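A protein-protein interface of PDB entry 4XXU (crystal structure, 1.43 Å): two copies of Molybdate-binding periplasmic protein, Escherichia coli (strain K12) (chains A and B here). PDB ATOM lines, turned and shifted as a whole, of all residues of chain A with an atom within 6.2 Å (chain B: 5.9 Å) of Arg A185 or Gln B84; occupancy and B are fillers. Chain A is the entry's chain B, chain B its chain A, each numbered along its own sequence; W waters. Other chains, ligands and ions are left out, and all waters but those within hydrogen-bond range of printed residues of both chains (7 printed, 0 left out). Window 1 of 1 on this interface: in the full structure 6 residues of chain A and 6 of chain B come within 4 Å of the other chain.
The side-chain amide nitrogen (NE2) of Gln B84 sits close to the guanidinium group (NH2) of Arg A185 (3.5 Å).
OG1 of Thr B98 sits at hydrogen-bond distance from ND2 of Asn A186, at 3.0 Å.
OE1 of Gln B84 lies within hydrogen-bond range of NH2 of Arg B101, 2.8 Å away.
The backbone carbonyl oxygen (O) of Leu A182 is in hydrogen-bond range of the backbone NH (N) of Glu A187, at 2.9 Å.
The side-chain carboxylate (OD1) of Asp B88 is in salt-bridge range of the guanidinium group (NH2) of Arg B101.
The side-chain amide nitrogen (NE2) of Gln B84 sits at hydrogen-bond distance from the side-chain hydroxyl (OG1) of Thr B103 (3.0 Å).
The side-chain carboxylate (OE1) of Glu B219 is in hydrogen-bond range of the side-chain amide nitrogen (NE2) of Gln B84 (3.0 Å).
Among the printed residues, pairs that only touch across the chains: Glu A187 with Arg B101 (3.5 Å) and Arg A185 with Arg B101 (3.6 Å).
Arg A185 touches just these residues of chain B: Gln B84 (3.4 Å) and Arg B101 (3.6 Å).
Of chain A, only Arg A185 (3.4 Å) comes within 4 Å of Gln B84.
Of the printed residues of chain A, Thr B98 touches Asn A186.
Printed residues of chain B within 4 Å of Glu A187: Arg B101 (3.5 Å).
Of the printed residues of chain A, Arg B101 touches Arg A185 and Glu A187.
Of the printed residues of chain B, Asn A186 touches Thr B98.
Leu A180 touches none of the printed residues of chain B.
Leu A182 touches none of the printed residues of chain B.
The nearest residue of chain B that does not touch Arg A185 is Thr B103 (4.2 Å).
The nearest residue of chain A that does not touch Gln B84 is Glu A187 (5.9 Å).
Printed residues of chain B that touch a printed residue of chain A: Gln B84, Thr B98 and Arg B101.
Along chain A the printed residues that touch a printed residue of chain B span positions 185 to 187.
Among the printed residues, 4 pairs touch across the chains.
No position is printed for both chains.
Water W1 bridges the side-chain carboxylate of Glu A187 (2.6 Å) and the backbone NH of Thr B103 (2.9 Å).
Water W3 lies within hydrogen-bond range of OE2 of Glu A187 (2.6 Å), OG1 of Thr B103 (2.8 Å) and NH2 of Arg A185 (3.1 Å).
Water W6 bridges OD2 of Asp B88 (2.7 Å) and NE of Arg A185 (2.8 Å).
Water W7 bridges the guanidinium group of Arg A185 (2.8 Å) and the side-chain carboxylate of Glu B219 (2.8 Å).
Water W2 lies within hydrogen-bond range of the backbone carbonyl oxygen of Arg A185 (2.8 Å) and the guanidinium group of Arg B101 (3.0 Å).
Water W4 lies within hydrogen-bond range of OE2 of Glu A187 (2.8 Å), NE of Arg B101 (2.9 Å) and OG1 of Thr B103 (3.0 Å).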
ATOM      1  N   GLY A 178     -20.569  24.362  23.256  1.00  0.00           N
ATOM      2  CA  GLY A 178     -20.080  24.304  21.890  1.00  0.00           C
ATOM      3  C   GLY A 178     -20.862  25.263  21.005  1.00  0.00           C
ATOM      4  O   GLY A 178     -20.308  25.894  20.100  1.00  0.00           O
ATOM      5  N   LEU A 180     -22.387  27.997  22.124  1.00  0.00           N
ATOM      6  CA  LEU A 180     -21.954  29.318  22.566  1.00  0.00           C
ATOM      7  C   LEU A 180     -20.631  29.675  21.911  1.00  0.00           C
ATOM      8  O   LEU A 180     -20.452  30.808  21.437  1.00  0.00           O
ATOM      9  CB  LEU A 180     -21.802  29.335  24.087  1.00  0.00           C
ATOM     10  CG  LEU A 180     -21.248  30.625  24.693  1.00  0.00           C
ATOM     11  CD1 LEU A 180     -22.252  31.745  24.523  1.00  0.00           C
ATOM     12  CD2 LEU A 180     -20.905  30.433  26.161  1.00  0.00           C
ATOM     13  N   ALA A 181     -19.717  28.705  21.867  1.00  0.00           N
ATOM     14  CA  ALA A 181     -18.401  28.930  21.258  1.00  0.00           C
ATOM     15  C   ALA A 181     -18.487  29.299  19.784  1.00  0.00           C
ATOM     16  O   ALA A 181     -17.723  30.144  19.323  1.00  0.00           O
ATOM     17  CB  ALA A 181     -17.508  27.716  21.452  1.00  0.00           C
ATOM     18  N   LEU A 182     -19.414  28.700  19.038  1.00  0.00           N
ATOM     19  CA  LEU A 182     -19.554  29.063  17.619  1.00  0.00           C
ATOM     20  C   LEU A 182     -19.905  30.538  17.449  1.00  0.00           C
ATOM     21  O   LEU A 182     -19.436  31.197  16.516  1.00  0.00           O
ATOM     22  CB  LEU A 182     -20.613  28.207  16.935  1.00  0.00           C
ATOM     23  CG  LEU A 182     -20.231  26.742  16.748  1.00  0.00           C
ATOM     24  CD1 LEU A 182     -21.406  25.985  16.160  1.00  0.00           C
ATOM     25  CD2 LEU A 182     -19.005  26.599  15.859  1.00  0.00           C
ATOM     26  N   VAL A 183     -20.707  31.071  18.364  1.00  0.00           N
ATOM     27  CA  VAL A 183     -21.082  32.482  18.304  1.00  0.00           C
ATOM     28  C   VAL A 183     -19.936  33.360  18.790  1.00  0.00           C
ATOM     29  O   VAL A 183     -19.600  34.364  18.141  1.00  0.00           O
ATOM     30  CB  VAL A 183     -22.355  32.763  19.128  1.00  0.00           C
ATOM     31  CG1 VAL A 183     -22.773  34.214  18.978  1.00  0.00           C
ATOM     32  CG2 VAL A 183     -23.485  31.842  18.677  1.00  0.00           C
ATOM     33  N   GLU A 184     -19.329  32.986  19.913  1.00  0.00           N
ATOM     34  CA  GLU A 184     -18.160  33.705  20.432  1.00  0.00           C
ATOM     35  C   GLU A 184     -17.079  33.841  19.355  1.00  0.00           C
ATOM     36  O   GLU A 184     -16.455  34.898  19.233  1.00  0.00           O
ATOM     37  CB  GLU A 184     -17.592  32.999  21.674  1.00  0.00           C
ATOM     38  CG  GLU A 184     -18.482  33.112  22.915  1.00  0.00           C
ATOM     39  CD  GLU A 184     -17.974  32.307  24.092  1.00  0.00           C
ATOM     40  OE1 GLU A 184     -17.503  31.170  23.886  1.00  0.00           O
ATOM     41  OE2 GLU A 184     -18.059  32.799  25.238  1.00  0.00           O
ATOM     42  N   ARG A 185     -16.886  32.786  18.565  1.00  0.00           N
ATOM     43  CA  ARG A 185     -15.837  32.744  17.540  1.00  0.00           C
ATOM     44  C   ARG A 185     -16.268  33.331  16.191  1.00  0.00           C
ATOM     45  O   ARG A 185     -15.513  33.277  15.208  1.00  0.00           O
ATOM     46  CB  ARG A 185     -15.344  31.304  17.361  1.00  0.00           C
ATOM     47  CG  ARG A 185     -14.747  30.709  18.640  1.00  0.00           C
ATOM     48  CD  ARG A 185     -14.530  29.205  18.556  1.00  0.00           C
ATOM     49  NE  ARG A 185     -14.072  28.674  19.838  1.00  0.00           N
ATOM     50  CZ  ARG A 185     -14.092  27.391  20.180  1.00  0.00           C
ATOM     51  NH1 ARG A 185     -13.660  27.027  21.377  1.00  0.00           N
ATOM     52  NH2 ARG A 185     -14.556  26.477  19.344  1.00  0.00           N
ATOM     53  N   ASN A 186     -17.470  33.898  16.147  1.00  0.00           N
ATOM     54  CA  ASN A 186     -18.045  34.465  14.917  1.00  0.00           C
ATOM     55  C   ASN A 186     -18.184  33.476  13.758  1.00  0.00           C
ATOM     56  O   ASN A 186     -18.208  33.862  12.585  1.00  0.00           O
ATOM     57  CB  ASN A 186     -17.319  35.746  14.469  1.00  0.00           C
ATOM     58  CG  ASN A 186     -18.218  36.665  13.647  1.00  0.00           C
ATOM     59  OD1 ASN A 186     -19.440  36.710  13.849  1.00  0.00           O
ATOM     60  ND2 ASN A 186     -17.622  37.389  12.705  1.00  0.00           N
ATOM     61  N   GLU A 187     -18.286  32.193  14.091  1.00  0.00           N
ATOM     62  CA  GLU A 187     -18.540  31.166  13.097  1.00  0.00           C
ATOM     63  C   GLU A 187     -20.027  31.049  12.772  1.00  0.00           C
ATOM     64  O   GLU A 187     -20.397  30.521  11.724  1.00  0.00           O
ATOM     65  CB  GLU A 187     -17.978  29.825  13.572  1.00  0.00           C
ATOM     66  CG  GLU A 187     -16.467  29.833  13.755  1.00  0.00           C
ATOM     67  CD  GLU A 187     -15.920  28.465  14.100  1.00  0.00           C
ATOM     68  OE1 GLU A 187     -16.210  27.512  13.353  1.00  0.00           O
ATOM     69  OE2 GLU A 187     -15.201  28.339  15.113  1.00  0.00           O
ATOM     70  N   ALA A 188     -20.869  31.527  13.683  1.00  0.00           N
ATOM     71  CA  ALA A 188     -22.304  31.632  13.444  1.00  0.00           C
ATOM     72  C   ALA A 188     -22.733  32.969  14.012  1.00  0.00           C
ATOM     73  O   ALA A 188     -22.285  33.354  15.091  1.00  0.00           O
ATOM     74  CB  ALA A 188     -23.059  30.495  14.138  1.00  0.00           C
ATOM     75  N   SER B  81      -3.233  27.983  15.297  1.00  0.00           N
ATOM     76  CA  SER B  81      -2.879  27.893  16.704  1.00  0.00           C
ATOM     77  C   SER B  81      -3.119  26.476  17.216  1.00  0.00           C
ATOM     78  O   SER B  81      -3.994  25.773  16.697  1.00  0.00           O
ATOM     79  CB  SER B  81      -3.767  28.870  17.490  1.00  0.00           C
ATOM     80  OG  SER B  81      -3.501  28.833  18.879  1.00  0.00           O
ATOM     81  N   ALA B  82      -2.371  26.065  18.238  1.00  0.00           N
ATOM     82  CA  ALA B  82      -2.587  24.758  18.883  1.00  0.00           C
ATOM     83  C   ALA B  82      -3.626  24.830  19.995  1.00  0.00           C
ATOM     84  O   ALA B  82      -3.902  23.829  20.654  1.00  0.00           O
ATOM     85  CB  ALA B  82      -1.285  24.197  19.430  1.00  0.00           C
ATOM     86  N   ASP B  83      -4.192  26.015  20.213  1.00  0.00           N
ATOM     87  CA  ASP B  83      -5.343  26.155  21.108  1.00  0.00           C
ATOM     88  C   ASP B  83      -6.299  27.254  20.666  1.00  0.00           C
ATOM     89  O   ASP B  83      -5.951  28.120  19.853  1.00  0.00           O
ATOM     90  CB  ASP B  83      -4.925  26.282  22.590  1.00  0.00           C
ATOM     91  CG  ASP B  83      -4.174  27.566  22.919  1.00  0.00           C
ATOM     92  OD1 ASP B  83      -4.169  28.512  22.109  1.00  0.00           O
ATOM     93  OD2 ASP B  83      -3.595  27.644  24.037  1.00  0.00           O
ATOM     94  N   GLN B  84      -7.517  27.195  21.188  1.00  0.00           N
ATOM     95  CA  GLN B  84      -8.486  28.235  20.921  1.00  0.00           C
ATOM     96  C   GLN B  84      -8.053  29.536  21.593  1.00  0.00           C
ATOM     97  O   GLN B  84      -8.260  30.623  21.026  1.00  0.00           O
ATOM     98  CB  GLN B  84      -9.862  27.799  21.438  1.00  0.00           C
ATOM     99  CG  GLN B  84     -10.382  26.497  20.833  1.00  0.00           C
ATOM    100  CD  GLN B  84     -10.780  26.593  19.354  1.00  0.00           C
ATOM    101  OE1 GLN B  84     -10.638  27.638  18.708  1.00  0.00           O
ATOM    102  NE2 GLN B  84     -11.279  25.488  18.814  1.00  0.00           N
ATOM    103  N   LYS B  85      -7.444  29.427  22.778  1.00  0.00           N
ATOM    104  CA  LYS B  85      -7.029  30.595  23.567  1.00  0.00           C
ATOM    105  C   LYS B  85      -6.264  31.644  22.760  1.00  0.00           C
ATOM    106  O   LYS B  85      -6.616  32.831  22.766  1.00  0.00           O
ATOM    107  CB  LYS B  85      -6.182  30.147  24.767  1.00  0.00           C
ATOM    108  CG  LYS B  85      -5.530  31.287  25.539  1.00  0.00           C
ATOM    109  CD  LYS B  85      -4.599  30.736  26.617  1.00  0.00           C
ATOM    110  CE  LYS B  85      -3.828  31.848  27.310  1.00  0.00           C
ATOM    111  NZ  LYS B  85      -4.691  32.667  28.206  1.00  0.00           N
ATOM    112  N   TRP B  86      -5.228  31.220  22.050  1.00  0.00           N
ATOM    113  CA  TRP B  86      -4.370  32.192  21.390  1.00  0.00           C
ATOM    114  C   TRP B  86      -4.952  32.703  20.086  1.00  0.00           C
ATOM    115  O   TRP B  86      -4.627  33.805  19.648  1.00  0.00           O
ATOM    116  CB  TRP B  86      -2.941  31.657  21.239  1.00  0.00           C
ATOM    117  CG  TRP B  86      -2.227  31.729  22.547  1.00  0.00           C
ATOM    118  CD1 TRP B  86      -1.919  30.679  23.379  1.00  0.00           C
ATOM    119  CD2 TRP B  86      -1.778  32.918  23.213  1.00  0.00           C
ATOM    120  NE1 TRP B  86      -1.290  31.149  24.509  1.00  0.00           N
ATOM    121  CE2 TRP B  86      -1.191  32.519  24.430  1.00  0.00           C
ATOM    122  CE3 TRP B  86      -1.801  34.281  22.890  1.00  0.00           C
ATOM    123  CZ2 TRP B  86      -0.633  33.434  25.325  1.00  0.00           C
ATOM    124  CZ3 TRP B  86      -1.245  35.187  23.780  1.00  0.00           C
ATOM    125  CH2 TRP B  86      -0.667  34.758  24.982  1.00  0.00           C
ATOM    126  N   MET B  87      -5.845  31.932  19.473  1.00  0.00           N
ATOM    127  CA  MET B  87      -6.642  32.476  18.377  1.00  0.00           C
ATOM    128  C   MET B  87      -7.631  33.515  18.900  1.00  0.00           C
ATOM    129  O   MET B  87      -7.765  34.593  18.304  1.00  0.00           O
ATOM    130  CB  MET B  87      -7.373  31.376  17.607  1.00  0.00           C
ATOM    131  CG  MET B  87      -8.170  31.911  16.421  1.00  0.00           C
ATOM    132  SD  MET B  87      -7.150  32.615  15.092  1.00  0.00           S
ATOM    133  CE  MET B  87      -6.403  31.133  14.410  1.00  0.00           C
ATOM    134  N   ASP B  88      -8.285  33.219  20.026  1.00  0.00           N
ATOM    135  CA  ASP B  88      -9.204  34.188  20.626  1.00  0.00           C
ATOM    136  C   ASP B  88      -8.455  35.469  20.944  1.00  0.00           C
ATOM    137  O   ASP B  88      -8.978  36.572  20.766  1.00  0.00           O
ATOM    138  CB  ASP B  88      -9.817  33.620  21.915  1.00  0.00           C
ATOM    139  CG  ASP B  88     -10.771  32.462  21.664  1.00  0.00           C
ATOM    140  OD1 ASP B  88     -11.287  32.328  20.533  1.00  0.00           O
ATOM    141  OD2 ASP B  88     -11.016  31.673  22.609  1.00  0.00           O
ATOM    142  N   TYR B  89      -7.212  35.331  21.393  1.00  0.00           N
ATOM    143  CA  TYR B  89      -6.397  36.482  21.725  1.00  0.00           C
ATOM    144  C   TYR B  89      -6.168  37.342  20.489  1.00  0.00           C
ATOM    145  O   TYR B  89      -6.379  38.560  20.513  1.00  0.00           O
ATOM    146  CB  TYR B  89      -5.050  36.028  22.315  1.00  0.00           C
ATOM    147  CG  TYR B  89      -4.119  37.166  22.625  1.00  0.00           C
ATOM    148  CD1 TYR B  89      -4.125  37.765  23.875  1.00  0.00           C
ATOM    149  CD2 TYR B  89      -3.234  37.648  21.662  1.00  0.00           C
ATOM    150  CE1 TYR B  89      -3.275  38.819  24.160  1.00  0.00           C
ATOM    151  CE2 TYR B  89      -2.392  38.699  21.932  1.00  0.00           C
ATOM    152  CZ  TYR B  89      -2.420  39.278  23.181  1.00  0.00           C
ATOM    153  OH  TYR B  89      -1.574  40.335  23.449  1.00  0.00           O
ATOM    154  N   THR B  98     -12.187  37.305  10.902  1.00  0.00           N
ATOM    155  CA  THR B  98     -12.977  36.331  11.660  1.00  0.00           C
ATOM    156  C   THR B  98     -13.908  35.491  10.781  1.00  0.00           C
ATOM    157  O   THR B  98     -14.290  34.383  11.167  1.00  0.00           O
ATOM    158  CB  THR B  98     -13.767  36.974  12.816  1.00  0.00           C
ATOM    159  OG1 THR B  98     -14.668  37.959  12.296  1.00  0.00           O
ATOM    160  CG2 THR B  98     -12.828  37.630  13.812  1.00  0.00           C
ATOM    161  N   ARG B 101     -12.322  32.066  10.281  1.00  0.00           N
ATOM    162  CA  ARG B 101     -11.917  31.209  11.389  1.00  0.00           C
ATOM    163  C   ARG B 101     -12.705  29.908  11.445  1.00  0.00           C
ATOM    164  O   ARG B 101     -13.935  29.898  11.320  1.00  0.00           O
ATOM    165  CB  ARG B 101     -12.062  31.925  12.722  1.00  0.00           C
ATOM    166  CG  ARG B 101     -11.534  31.089  13.870  1.00  0.00           C
ATOM    167  CD  ARG B 101     -12.093  31.546  15.175  1.00  0.00           C
ATOM    168  NE  ARG B 101     -11.642  30.725  16.296  1.00  0.00           N
ATOM    169  CZ  ARG B 101     -11.418  31.218  17.502  1.00  0.00           C
ATOM    170  NH1 ARG B 101     -11.604  32.516  17.736  1.00  0.00           N
ATOM    171  NH2 ARG B 101     -11.011  30.421  18.478  1.00  0.00           N
ATOM    172  N   THR B 103     -12.233  25.601  13.299  1.00  0.00           N
ATOM    173  CA  THR B 103     -11.402  24.592  13.942  1.00  0.00           C
ATOM    174  C   THR B 103     -11.040  23.512  12.943  1.00  0.00           C
ATOM    175  O   THR B 103     -11.913  22.897  12.333  1.00  0.00           O
ATOM    176  CB  THR B 103     -12.120  23.987  15.141  1.00  0.00           C
ATOM    177  OG1 THR B 103     -12.429  25.037  16.058  1.00  0.00           O
ATOM    178  CG2 THR B 103     -11.222  22.971  15.830  1.00  0.00           C
ATOM    179  N   TYR B 152      -2.357  23.228  28.443  1.00  0.00           N
ATOM    180  CA  TYR B 152      -3.115  21.986  28.519  1.00  0.00           C
ATOM    181  C   TYR B 152      -2.562  21.098  29.629  1.00  0.00           C
ATOM    182  O   TYR B 152      -3.329  20.497  30.391  1.00  0.00           O
ATOM    183  CB  TYR B 152      -3.026  21.206  27.203  1.00  0.00           C
ATOM    184  CG  TYR B 152      -3.732  21.783  25.978  1.00  0.00           C
ATOM    185  CD1 TYR B 152      -5.112  21.943  25.939  1.00  0.00           C
ATOM    186  CD2 TYR B 152      -3.018  22.056  24.814  1.00  0.00           C
ATOM    187  CE1 TYR B 152      -5.752  22.428  24.801  1.00  0.00           C
ATOM    188  CE2 TYR B 152      -3.644  22.539  23.672  1.00  0.00           C
ATOM    189  CZ  TYR B 152      -5.014  22.727  23.672  1.00  0.00           C
ATOM    190  OH  TYR B 152      -5.668  23.188  22.537  1.00  0.00           O
ATOM    191  N   GLU B 219      -7.335  21.479  20.278  1.00  0.00           N
ATOM    192  CA  GLU B 219      -7.944  21.891  19.015  1.00  0.00           C
ATOM    193  C   GLU B 219      -7.117  22.966  18.357  1.00  0.00           C
ATOM    194  O   GLU B 219      -6.574  23.845  19.031  1.00  0.00           O
ATOM    195  CB  GLU B 219      -9.361  22.431  19.241  1.00  0.00           C
ATOM    196  CG  GLU B 219     -10.334  21.390  19.756  1.00  0.00           C
ATOM    197  CD  GLU B 219     -11.724  21.950  19.937  1.00  0.00           C
ATOM    198  OE1 GLU B 219     -11.850  23.061  20.489  1.00  0.00           O
ATOM    199  OE2 GLU B 219     -12.683  21.266  19.520  1.00  0.00           O
ATOM    200  N   TYR B 220      -7.048  22.892  17.035  1.00  0.00           N
ATOM    201  CA  TYR B 220      -6.264  23.833  16.242  1.00  0.00           C
ATOM    202  C   TYR B 220      -7.162  24.667  15.341  1.00  0.00           C
ATOM    203  O   TYR B 220      -7.567  24.193  14.282  1.00  0.00           O
ATOM    204  CB  TYR B 220      -5.268  23.088  15.334  1.00  0.00           C
ATOM    205  CG  TYR B 220      -4.151  22.371  16.053  1.00  0.00           C
ATOM    206  CD1 TYR B 220      -4.404  21.239  16.815  1.00  0.00           C
ATOM    207  CD2 TYR B 220      -2.838  22.806  15.942  1.00  0.00           C
ATOM    208  CE1 TYR B 220      -3.386  20.575  17.482  1.00  0.00           C
ATOM    209  CE2 TYR B 220      -1.801  22.137  16.604  1.00  0.00           C
ATOM    210  CZ  TYR B 220      -2.091  21.029  17.369  1.00  0.00           C
ATOM    211  OH  TYR B 220      -1.097  20.356  18.029  1.00  0.00           O
ATOM    212  N   PRO B 221      -7.462  25.913  15.742  1.00  0.00           N
ATOM    213  CA  PRO B 221      -8.155  26.824  14.820  1.00  0.00           C
ATOM    214  C   PRO B 221      -7.201  27.415  13.784  1.00  0.00           C
ATOM    215  O   PRO B 221      -6.013  27.645  14.051  1.00  0.00           O
ATOM    216  CB  PRO B 221      -8.685  27.922  15.748  1.00  0.00           C
ATOM    217  CG  PRO B 221      -7.675  27.979  16.846  1.00  0.00           C
ATOM    218  CD  PRO B 221      -7.190  26.541  17.044  1.00  0.00           C
HETATM  219  O   HOH W   1     -15.098  25.155  13.251  1.00  0.00           O
HETATM  220  O   HOH W   2     -13.105  34.449  15.969  1.00  0.00           O
HETATM  221  O   HOH W   3     -14.980  26.040  16.343  1.00  0.00           O
HETATM  222  O   HOH W   4     -12.479  28.031  15.632  1.00  0.00           O
HETATM  223  O   HOH W   5     -16.551  28.193  10.624  1.00  0.00           O
HETATM  224  O   HOH W   6     -12.926  29.807  22.162  1.00  0.00           O
HETATM  225  O   HOH W   7     -13.933  24.325  21.915  1.00  0.00           O
